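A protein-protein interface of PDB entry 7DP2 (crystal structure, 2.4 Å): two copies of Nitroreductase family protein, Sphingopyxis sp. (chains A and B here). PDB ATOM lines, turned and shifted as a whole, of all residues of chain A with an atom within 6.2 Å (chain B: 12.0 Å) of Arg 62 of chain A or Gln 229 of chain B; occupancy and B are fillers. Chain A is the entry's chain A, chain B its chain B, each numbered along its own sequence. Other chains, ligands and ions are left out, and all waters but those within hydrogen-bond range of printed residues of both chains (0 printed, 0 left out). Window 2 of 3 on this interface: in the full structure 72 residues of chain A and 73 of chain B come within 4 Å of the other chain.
No position is printed for both chains.
The backbone NH (N) of Val 57 of chain A sits at hydrogen-bond distance from the backbone carbonyl oxygen (O) of Asp 227 of chain B (2.7 Å). N of Gln 229 of chain B lies within hydrogen-bond range of O of Val 57 of chain A (2.8 Å). N of Thr 59 of chain A sits at hydrogen-bond distance from O of Gln 229 of chain B (3.0 Å). The side-chain amide oxygen (OE1) of Gln 229 of chain B is in hydrogen-bond range of the guanidinium group (NE) of Arg 62 of chain A, 3.2 Å away. O of Leu 189 of chain A is in hydrogen-bond range of NE2 of Gln 229 of chain B.
The side-chain amide nitrogen (NE2) of Gln 229 of chain B sits at hydrogen-bond distance from the side-chain carboxylate (OD2) of Asp 227 of chain B, at 2.9 Å.
Arg 62 of chain A touches just these residues of chain B: Gln 229 (3.2 Å) and Gly 230 (3.5 Å). Gln 229 of chain B touches just these residues of chain A: Thr 56 (3.6 Å), Val 57 (2.8 Å), Val 58 (3.2 Å), Thr 59 (3.0 Å), Arg 62 (3.2 Å) and Leu 189 (3.4 Å). Of chain B, only Ile 226 (3.7 Å), Asp 227 (2.7 Å), Trp 228 (3.6 Å), Gln 229 (2.8 Å) and Phe 231 (3.6 Å) come within 4 Å of Val 57 of chain A. Val 58 of chain A touches just one residue of chain B: Gln 229. Of chain B, only Gln 229 (3.0 Å), Gly 230 (3.1 Å) and Phe 231 (3.5 Å) come within 4 Å of Thr 59 of chain A. No residue of chain B comes within 4 Å of Gly 60 of chain A. Glu 61 of chain A touches none of the printed residues of chain B. Of chain B, only Gln 229 (3.4 Å) comes within 4 Å of Leu 189 of chain A. No residue of chain B comes within 4 Å of Gly 190 of chain A. Printed residues of chain A within 4 Å of Phe 231 of chain B: Val 57 (3.6 Å) and Thr 59 (3.5 Å). Of the printed residues of chain A, Gly 230 of chain B touches Thr 59 (3.1 Å) and Arg 62 (3.5 Å). Of the printed residues of chain A, Asp 227 of chain B touches Thr 56 and Val 57. Of the printed residues of chain A, Trp 228 of chain B touches Val 57 (3.6 Å). Of the printed residues of chain A, Ile 226 of chain B touches Val 57 (3.7 Å). Asp 223 of chain B touches none of the printed residues of chain A. Ala 187 of chain A touches none of the printed residues of chain B. The nearest residue of chain A that does not touch Gln 229 of chain B is Glu 188 of chain A (4.9 Å). The nearest printed residue of chain A that does not touch Phe 231 of chain B is Val 58 of chain A (4.7 Å).
Among the printed residues, merely in contact across the chains: Thr 59 of chain A with Gly 230 of chain B, Val 58 of chain A with Gln 229 of chain B, Thr 59 of chain A with Phe 231 of chain B, Arg 62 of chain A with Gly 230 of chain B, Thr 56 of chain A with Asp 227 of chain B, Val 57 of chain A with Phe 231 of chain B, Val 57 of chain A with Trp 228 of chain B, Thr 56 of chain A with Gln 229 of chain B and Val 57 of chain A with Ile 226 of chain B.
Hydrophobic or aromatic side chains of chain B that line the printed part of chain A: Ile 226 and Phe 231. Among the printed residues, 14 pairs touch across the chains. Among the printed residues, no Asp or Glu carboxylate lies within 4 Å of a Lys or Arg side-chain nitrogen of the other chain.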
ATOM      1  N   THR A  56     -20.445   4.549 -34.319  1.00  0.00           N
ATOM      2  CA  THR A  56     -20.013   4.124 -33.000  1.00  0.00           C
ATOM      3  C   THR A  56     -20.937   4.707 -31.930  1.00  0.00           C
ATOM      4  O   THR A  56     -21.093   5.912 -31.833  1.00  0.00           O
ATOM      5  CB  THR A  56     -18.566   4.550 -32.729  1.00  0.00           C
ATOM      6  OG1 THR A  56     -17.732   4.054 -33.784  1.00  0.00           O
ATOM      7  CG2 THR A  56     -18.094   3.998 -31.394  1.00  0.00           C
ATOM      8  N   VAL A  57     -21.550   3.845 -31.129  1.00  0.00           N
ATOM      9  CA  VAL A  57     -22.520   4.298 -30.135  1.00  0.00           C
ATOM     10  C   VAL A  57     -21.979   4.151 -28.729  1.00  0.00           C
ATOM     11  O   VAL A  57     -21.680   3.040 -28.288  1.00  0.00           O
ATOM     12  CB  VAL A  57     -23.829   3.499 -30.225  1.00  0.00           C
ATOM     13  CG1 VAL A  57     -24.832   4.035 -29.239  1.00  0.00           C
ATOM     14  CG2 VAL A  57     -24.373   3.570 -31.616  1.00  0.00           C
ATOM     15  N   VAL A  58     -21.883   5.260 -28.004  1.00  0.00           N
ATOM     16  CA  VAL A  58     -21.275   5.200 -26.684  1.00  0.00           C
ATOM     17  C   VAL A  58     -22.197   5.697 -25.577  1.00  0.00           C
ATOM     18  O   VAL A  58     -22.943   6.664 -25.741  1.00  0.00           O
ATOM     19  CB  VAL A  58     -19.949   5.985 -26.656  1.00  0.00           C
ATOM     20  CG1 VAL A  58     -18.975   5.415 -27.688  1.00  0.00           C
ATOM     21  CG2 VAL A  58     -20.198   7.451 -26.912  1.00  0.00           C
ATOM     22  N   THR A  59     -22.114   5.031 -24.433  1.00  0.00           N
ATOM     23  CA  THR A  59     -22.866   5.446 -23.267  1.00  0.00           C
ATOM     24  C   THR A  59     -22.018   5.245 -22.025  1.00  0.00           C
ATOM     25  O   THR A  59     -20.874   4.797 -22.125  1.00  0.00           O
ATOM     26  CB  THR A  59     -24.160   4.651 -23.117  1.00  0.00           C
ATOM     27  OG1 THR A  59     -25.015   5.300 -22.165  1.00  0.00           O
ATOM     28  CG2 THR A  59     -23.854   3.232 -22.649  1.00  0.00           C
ATOM     29  N   GLY A  60     -22.578   5.575 -20.864  1.00  0.00           N
ATOM     30  CA  GLY A  60     -21.897   5.365 -19.610  1.00  0.00           C
ATOM     31  C   GLY A  60     -20.592   6.128 -19.594  1.00  0.00           C
ATOM     32  O   GLY A  60     -20.547   7.328 -19.886  1.00  0.00           O
ATOM     33  N   GLU A  61     -19.511   5.419 -19.313  1.00  0.00           N
ATOM     34  CA  GLU A  61     -18.240   6.087 -19.085  1.00  0.00           C
ATOM     35  C   GLU A  61     -17.263   5.878 -20.229  1.00  0.00           C
ATOM     36  O   GLU A  61     -16.131   6.353 -20.189  1.00  0.00           O
ATOM     37  CB  GLU A  61     -17.629   5.666 -17.751  1.00  0.00           C
ATOM     38  CG  GLU A  61     -18.528   5.950 -16.590  1.00  0.00           C
ATOM     39  CD  GLU A  61     -17.857   5.795 -15.254  1.00  0.00           C
ATOM     40  OE1 GLU A  61     -16.905   6.549 -14.984  1.00  0.00           O
ATOM     41  OE2 GLU A  61     -18.253   4.891 -14.499  1.00  0.00           O
ATOM     42  N   ARG A  62     -17.694   5.155 -21.247  1.00  0.00           N
ATOM     43  CA  ARG A  62     -16.983   5.226 -22.506  1.00  0.00           C
ATOM     44  C   ARG A  62     -17.310   6.607 -23.058  1.00  0.00           C
ATOM     45  O   ARG A  62     -16.459   7.330 -23.587  1.00  0.00           O
ATOM     46  CB  ARG A  62     -17.434   4.122 -23.460  1.00  0.00           C
ATOM     47  CG  ARG A  62     -16.682   2.812 -23.286  1.00  0.00           C
ATOM     48  CD  ARG A  62     -15.204   3.064 -23.466  1.00  0.00           C
ATOM     49  NE  ARG A  62     -14.976   3.927 -24.622  1.00  0.00           N
ATOM     50  CZ  ARG A  62     -13.839   4.565 -24.870  1.00  0.00           C
ATOM     51  NH1 ARG A  62     -13.733   5.320 -25.952  1.00  0.00           N
ATOM     52  NH2 ARG A  62     -12.810   4.456 -24.041  1.00  0.00           N
ATOM     53  N   TRP A  63     -18.567   6.963 -22.861  1.00  0.00           N
ATOM     54  CA  TRP A  63     -19.138   8.232 -23.236  1.00  0.00           C
ATOM     55  C   TRP A  63     -18.636   9.346 -22.304  1.00  0.00           C
ATOM     56  O   TRP A  63     -18.501  10.504 -22.705  1.00  0.00           O
ATOM     57  CB  TRP A  63     -20.660   8.077 -23.235  1.00  0.00           C
ATOM     58  CG  TRP A  63     -21.483   9.299 -23.278  1.00  0.00           C
ATOM     59  CD1 TRP A  63     -22.612   9.523 -22.559  1.00  0.00           C
ATOM     60  CD2 TRP A  63     -21.276  10.466 -24.092  1.00  0.00           C
ATOM     61  NE1 TRP A  63     -23.118  10.768 -22.856  1.00  0.00           N
ATOM     62  CE2 TRP A  63     -22.316  11.372 -23.791  1.00  0.00           C
ATOM     63  CE3 TRP A  63     -20.313  10.847 -25.037  1.00  0.00           C
ATOM     64  CZ2 TRP A  63     -22.424  12.629 -24.396  1.00  0.00           C
ATOM     65  CZ3 TRP A  63     -20.412  12.108 -25.639  1.00  0.00           C
ATOM     66  CH2 TRP A  63     -21.462  12.981 -25.312  1.00  0.00           C
ATOM     67  N   GLN A  64     -18.369   8.999 -21.053  1.00  0.00           N
ATOM     68  CA  GLN A  64     -17.815   9.987 -20.142  1.00  0.00           C
ATOM     69  C   GLN A  64     -16.369  10.284 -20.498  1.00  0.00           C
ATOM     70  O   GLN A  64     -15.940  11.425 -20.434  1.00  0.00           O
ATOM     71  CB  GLN A  64     -17.910   9.508 -18.692  1.00  0.00           C
ATOM     72  CG  GLN A  64     -17.303  10.469 -17.700  1.00  0.00           C
ATOM     73  CD  GLN A  64     -18.124  11.734 -17.589  1.00  0.00           C
ATOM     74  OE1 GLN A  64     -19.158  11.758 -16.921  1.00  0.00           O
ATOM     75  NE2 GLN A  64     -17.675  12.791 -18.254  1.00  0.00           N
ATOM     76  N   ALA A  65     -15.638   9.245 -20.898  1.00  0.00           N
ATOM     77  CA  ALA A  65     -14.253   9.373 -21.355  1.00  0.00           C
ATOM     78  C   ALA A  65     -14.126  10.386 -22.498  1.00  0.00           C
ATOM     79  O   ALA A  65     -13.239  11.240 -22.484  1.00  0.00           O
ATOM     80  CB  ALA A  65     -13.722   8.022 -21.798  1.00  0.00           C
ATOM     81  N   VAL A  66     -15.016  10.281 -23.480  1.00  0.00           N
ATOM     82  CA  VAL A  66     -15.026  11.197 -24.615  1.00  0.00           C
ATOM     83  C   VAL A  66     -15.244  12.636 -24.168  1.00  0.00           C
ATOM     84  O   VAL A  66     -14.534  13.551 -24.593  1.00  0.00           O
ATOM     85  CB  VAL A  66     -16.129  10.824 -25.639  1.00  0.00           C
ATOM     86  CG1 VAL A  66     -16.306  11.921 -26.667  1.00  0.00           C
ATOM     87  CG2 VAL A  66     -15.823   9.488 -26.303  1.00  0.00           C
ATOM     88  N   GLN A  67     -16.238  12.832 -23.317  1.00  0.00           N
ATOM     89  CA  GLN A  67     -16.543  14.159 -22.820  1.00  0.00           C
ATOM     90  C   GLN A  67     -15.341  14.790 -22.146  1.00  0.00           C
ATOM     91  O   GLN A  67     -15.019  15.942 -22.406  1.00  0.00           O
ATOM     92  CB  GLN A  67     -17.718  14.097 -21.850  1.00  0.00           C
ATOM     93  CG  GLN A  67     -19.033  13.787 -22.537  1.00  0.00           C
ATOM     94  CD  GLN A  67     -20.122  13.468 -21.557  1.00  0.00           C
ATOM     95  OE1 GLN A  67     -20.720  14.361 -20.975  1.00  0.00           O
ATOM     96  NE2 GLN A  67     -20.394  12.183 -21.373  1.00  0.00           N
ATOM     97  N   ALA A 187      -9.684   9.204 -31.429  1.00  0.00           N
ATOM     98  CA  ALA A 187      -8.738   8.547 -30.536  1.00  0.00           C
ATOM     99  C   ALA A 187      -9.439   7.843 -29.390  1.00  0.00           C
ATOM    100  O   ALA A 187      -9.177   6.674 -29.116  1.00  0.00           O
ATOM    101  CB  ALA A 187      -7.738   9.546 -29.995  1.00  0.00           C
ATOM    102  N   GLU A 188     -10.315   8.563 -28.706  1.00  0.00           N
ATOM    103  CA  GLU A 188     -11.031   7.987 -27.578  1.00  0.00           C
ATOM    104  C   GLU A 188     -11.827   6.762 -27.995  1.00  0.00           C
ATOM    105  O   GLU A 188     -11.906   5.775 -27.269  1.00  0.00           O
ATOM    106  CB  GLU A 188     -11.951   9.029 -26.962  1.00  0.00           C
ATOM    107  CG  GLU A 188     -11.176  10.134 -26.327  1.00  0.00           C
ATOM    108  CD  GLU A 188     -10.247   9.601 -25.259  1.00  0.00           C
ATOM    109  OE1 GLU A 188     -10.674   8.670 -24.539  1.00  0.00           O
ATOM    110  OE2 GLU A 188      -9.100  10.100 -25.139  1.00  0.00           O
ATOM    111  N   LEU A 189     -12.404   6.851 -29.184  1.00  0.00           N
ATOM    112  CA  LEU A 189     -13.217   5.798 -29.769  1.00  0.00           C
ATOM    113  C   LEU A 189     -12.391   4.665 -30.346  1.00  0.00           C
ATOM    114  O   LEU A 189     -12.891   3.551 -30.509  1.00  0.00           O
ATOM    115  CB  LEU A 189     -14.103   6.390 -30.864  1.00  0.00           C
ATOM    116  CG  LEU A 189     -15.561   6.676 -30.513  1.00  0.00           C
ATOM    117  CD1 LEU A 189     -15.728   7.165 -29.086  1.00  0.00           C
ATOM    118  CD2 LEU A 189     -16.193   7.621 -31.541  1.00  0.00           C
ATOM    119  N   GLY A 190     -11.140   4.959 -30.685  1.00  0.00           N
ATOM    120  CA  GLY A 190     -10.257   3.950 -31.239  1.00  0.00           C
ATOM    121  C   GLY A 190     -10.363   3.715 -32.739  1.00  0.00           C
ATOM    122  O   GLY A 190      -9.972   2.652 -33.218  1.00  0.00           O
ATOM    123  N   LEU B 222     -26.109  -5.290 -39.330  1.00  0.00           N
ATOM    124  CA  LEU B 222     -25.663  -4.222 -38.445  1.00  0.00           C
ATOM    125  C   LEU B 222     -24.285  -4.427 -37.838  1.00  0.00           C
ATOM    126  O   LEU B 222     -23.653  -3.466 -37.422  1.00  0.00           O
ATOM    127  CB  LEU B 222     -26.681  -4.003 -37.343  1.00  0.00           C
ATOM    128  CG  LEU B 222     -27.549  -2.774 -37.570  1.00  0.00           C
ATOM    129  CD1 LEU B 222     -28.110  -2.692 -38.959  1.00  0.00           C
ATOM    130  CD2 LEU B 222     -28.668  -2.816 -36.552  1.00  0.00           C
ATOM    131  N   ASP B 223     -23.804  -5.662 -37.798  1.00  0.00           N
ATOM    132  CA  ASP B 223     -22.461  -5.907 -37.284  1.00  0.00           C
ATOM    133  C   ASP B 223     -21.390  -5.296 -38.202  1.00  0.00           C
ATOM    134  O   ASP B 223     -20.233  -5.157 -37.816  1.00  0.00           O
ATOM    135  CB  ASP B 223     -22.243  -7.405 -37.043  1.00  0.00           C
ATOM    136  CG  ASP B 223     -22.728  -8.262 -38.189  1.00  0.00           C
ATOM    137  OD1 ASP B 223     -23.752  -7.909 -38.814  1.00  0.00           O
ATOM    138  OD2 ASP B 223     -22.154  -9.341 -38.412  1.00  0.00           O
ATOM    139  N   VAL B 225     -21.944  -2.290 -39.301  1.00  0.00           N
ATOM    140  CA  VAL B 225     -22.385  -0.912 -39.290  1.00  0.00           C
ATOM    141  C   VAL B 225     -22.260  -0.212 -37.938  1.00  0.00           C
ATOM    142  O   VAL B 225     -21.830   0.942 -37.863  1.00  0.00           O
ATOM    143  CB  VAL B 225     -23.871  -0.821 -39.734  1.00  0.00           C
ATOM    144  CG1 VAL B 225     -24.383   0.633 -39.715  1.00  0.00           C
ATOM    145  CG2 VAL B 225     -24.075  -1.502 -41.066  1.00  0.00           C
ATOM    146  N   ILE B 226     -22.690  -0.896 -36.881  1.00  0.00           N
ATOM    147  CA  ILE B 226     -22.826  -0.267 -35.573  1.00  0.00           C
ATOM    148  C   ILE B 226     -21.912  -0.900 -34.547  1.00  0.00           C
ATOM    149  O   ILE B 226     -21.957  -2.103 -34.353  1.00  0.00           O
ATOM    150  CB  ILE B 226     -24.267  -0.348 -35.025  1.00  0.00           C
ATOM    151  CG1 ILE B 226     -25.277   0.069 -36.082  1.00  0.00           C
ATOM    152  CG2 ILE B 226     -24.423   0.542 -33.780  1.00  0.00           C
ATOM    153  CD1 ILE B 226     -25.285   1.552 -36.328  1.00  0.00           C
ATOM    154  N   ASP B 227     -21.084  -0.073 -33.909  1.00  0.00           N
ATOM    155  CA  ASP B 227     -20.266  -0.473 -32.760  1.00  0.00           C
ATOM    156  C   ASP B 227     -20.882   0.034 -31.459  1.00  0.00           C
ATOM    157  O   ASP B 227     -21.257   1.207 -31.363  1.00  0.00           O
ATOM    158  CB  ASP B 227     -18.854   0.056 -32.906  1.00  0.00           C
ATOM    159  CG  ASP B 227     -17.933  -0.480 -31.861  1.00  0.00           C
ATOM    160  OD1 ASP B 227     -18.169  -1.612 -31.386  1.00  0.00           O
ATOM    161  OD2 ASP B 227     -16.987   0.248 -31.495  1.00  0.00           O
ATOM    162  N   TRP B 228     -20.987  -0.834 -30.460  1.00  0.00           N
ATOM    163  CA  TRP B 228     -21.554  -0.453 -29.173  1.00  0.00           C
ATOM    164  C   TRP B 228     -20.463  -0.399 -28.101  1.00  0.00           C
ATOM    165  O   TRP B 228     -19.726  -1.371 -27.891  1.00  0.00           O
ATOM    166  CB  TRP B 228     -22.650  -1.446 -28.763  1.00  0.00           C
ATOM    167  CG  TRP B 228     -23.683  -1.715 -29.842  1.00  0.00           C
ATOM    168  CD1 TRP B 228     -23.541  -2.553 -30.901  1.00  0.00           C
ATOM    169  CD2 TRP B 228     -25.013  -1.173 -29.939  1.00  0.00           C
ATOM    170  NE1 TRP B 228     -24.680  -2.552 -31.668  1.00  0.00           N
ATOM    171  CE2 TRP B 228     -25.595  -1.715 -31.099  1.00  0.00           C
ATOM    172  CE3 TRP B 228     -25.751  -0.272 -29.172  1.00  0.00           C
ATOM    173  CZ2 TRP B 228     -26.888  -1.396 -31.498  1.00  0.00           C
ATOM    174  CZ3 TRP B 228     -27.030   0.043 -29.572  1.00  0.00           C
ATOM    175  CH2 TRP B 228     -27.589  -0.519 -30.723  1.00  0.00           C
ATOM    176  N   GLN B 229     -20.362   0.742 -27.422  1.00  0.00           N
ATOM    177  CA  GLN B 229     -19.400   0.914 -26.328  1.00  0.00           C
ATOM    178  C   GLN B 229     -20.030   1.532 -25.084  1.00  0.00           C
ATOM    179  O   GLN B 229     -20.837   2.464 -25.183  1.00  0.00           O
ATOM    180  CB  GLN B 229     -18.243   1.800 -26.768  1.00  0.00           C
ATOM    181  CG  GLN B 229     -17.696   1.517 -28.147  1.00  0.00           C
ATOM    182  CD  GLN B 229     -16.384   2.238 -28.361  1.00  0.00           C
ATOM    183  OE1 GLN B 229     -15.953   3.005 -27.502  1.00  0.00           O
ATOM    184  NE2 GLN B 229     -15.746   2.004 -29.502  1.00  0.00           N
ATOM    185  N   GLY B 230     -19.617   1.049 -23.914  1.00  0.00           N
ATOM    186  CA  GLY B 230     -20.091   1.587 -22.652  1.00  0.00           C
ATOM    187  C   GLY B 230     -21.344   0.891 -22.168  1.00  0.00           C
ATOM    188  O   GLY B 230     -21.948   1.305 -21.173  1.00  0.00           O
ATOM    189  N   PHE B 231     -21.721  -0.188 -22.855  1.00  0.00           N
ATOM    190  CA  PHE B 231     -22.861  -1.006 -22.448  1.00  0.00           C
ATOM    191  C   PHE B 231     -22.421  -2.271 -21.719  1.00  0.00           C
ATOM    192  O   PHE B 231     -23.129  -3.285 -21.744  1.00  0.00           O
ATOM    193  CB  PHE B 231     -23.699  -1.384 -23.661  1.00  0.00           C
ATOM    194  CG  PHE B 231     -24.239  -0.210 -24.409  1.00  0.00           C
ATOM    195  CD1 PHE B 231     -25.449   0.350 -24.045  1.00  0.00           C
ATOM    196  CD2 PHE B 231     -23.550   0.324 -25.486  1.00  0.00           C
ATOM    197  CE1 PHE B 231     -25.962   1.428 -24.728  1.00  0.00           C
ATOM    198  CE2 PHE B 231     -24.056   1.403 -26.181  1.00  0.00           C
ATOM    199  CZ  PHE B 231     -25.269   1.957 -25.804  1.00  0.00           C
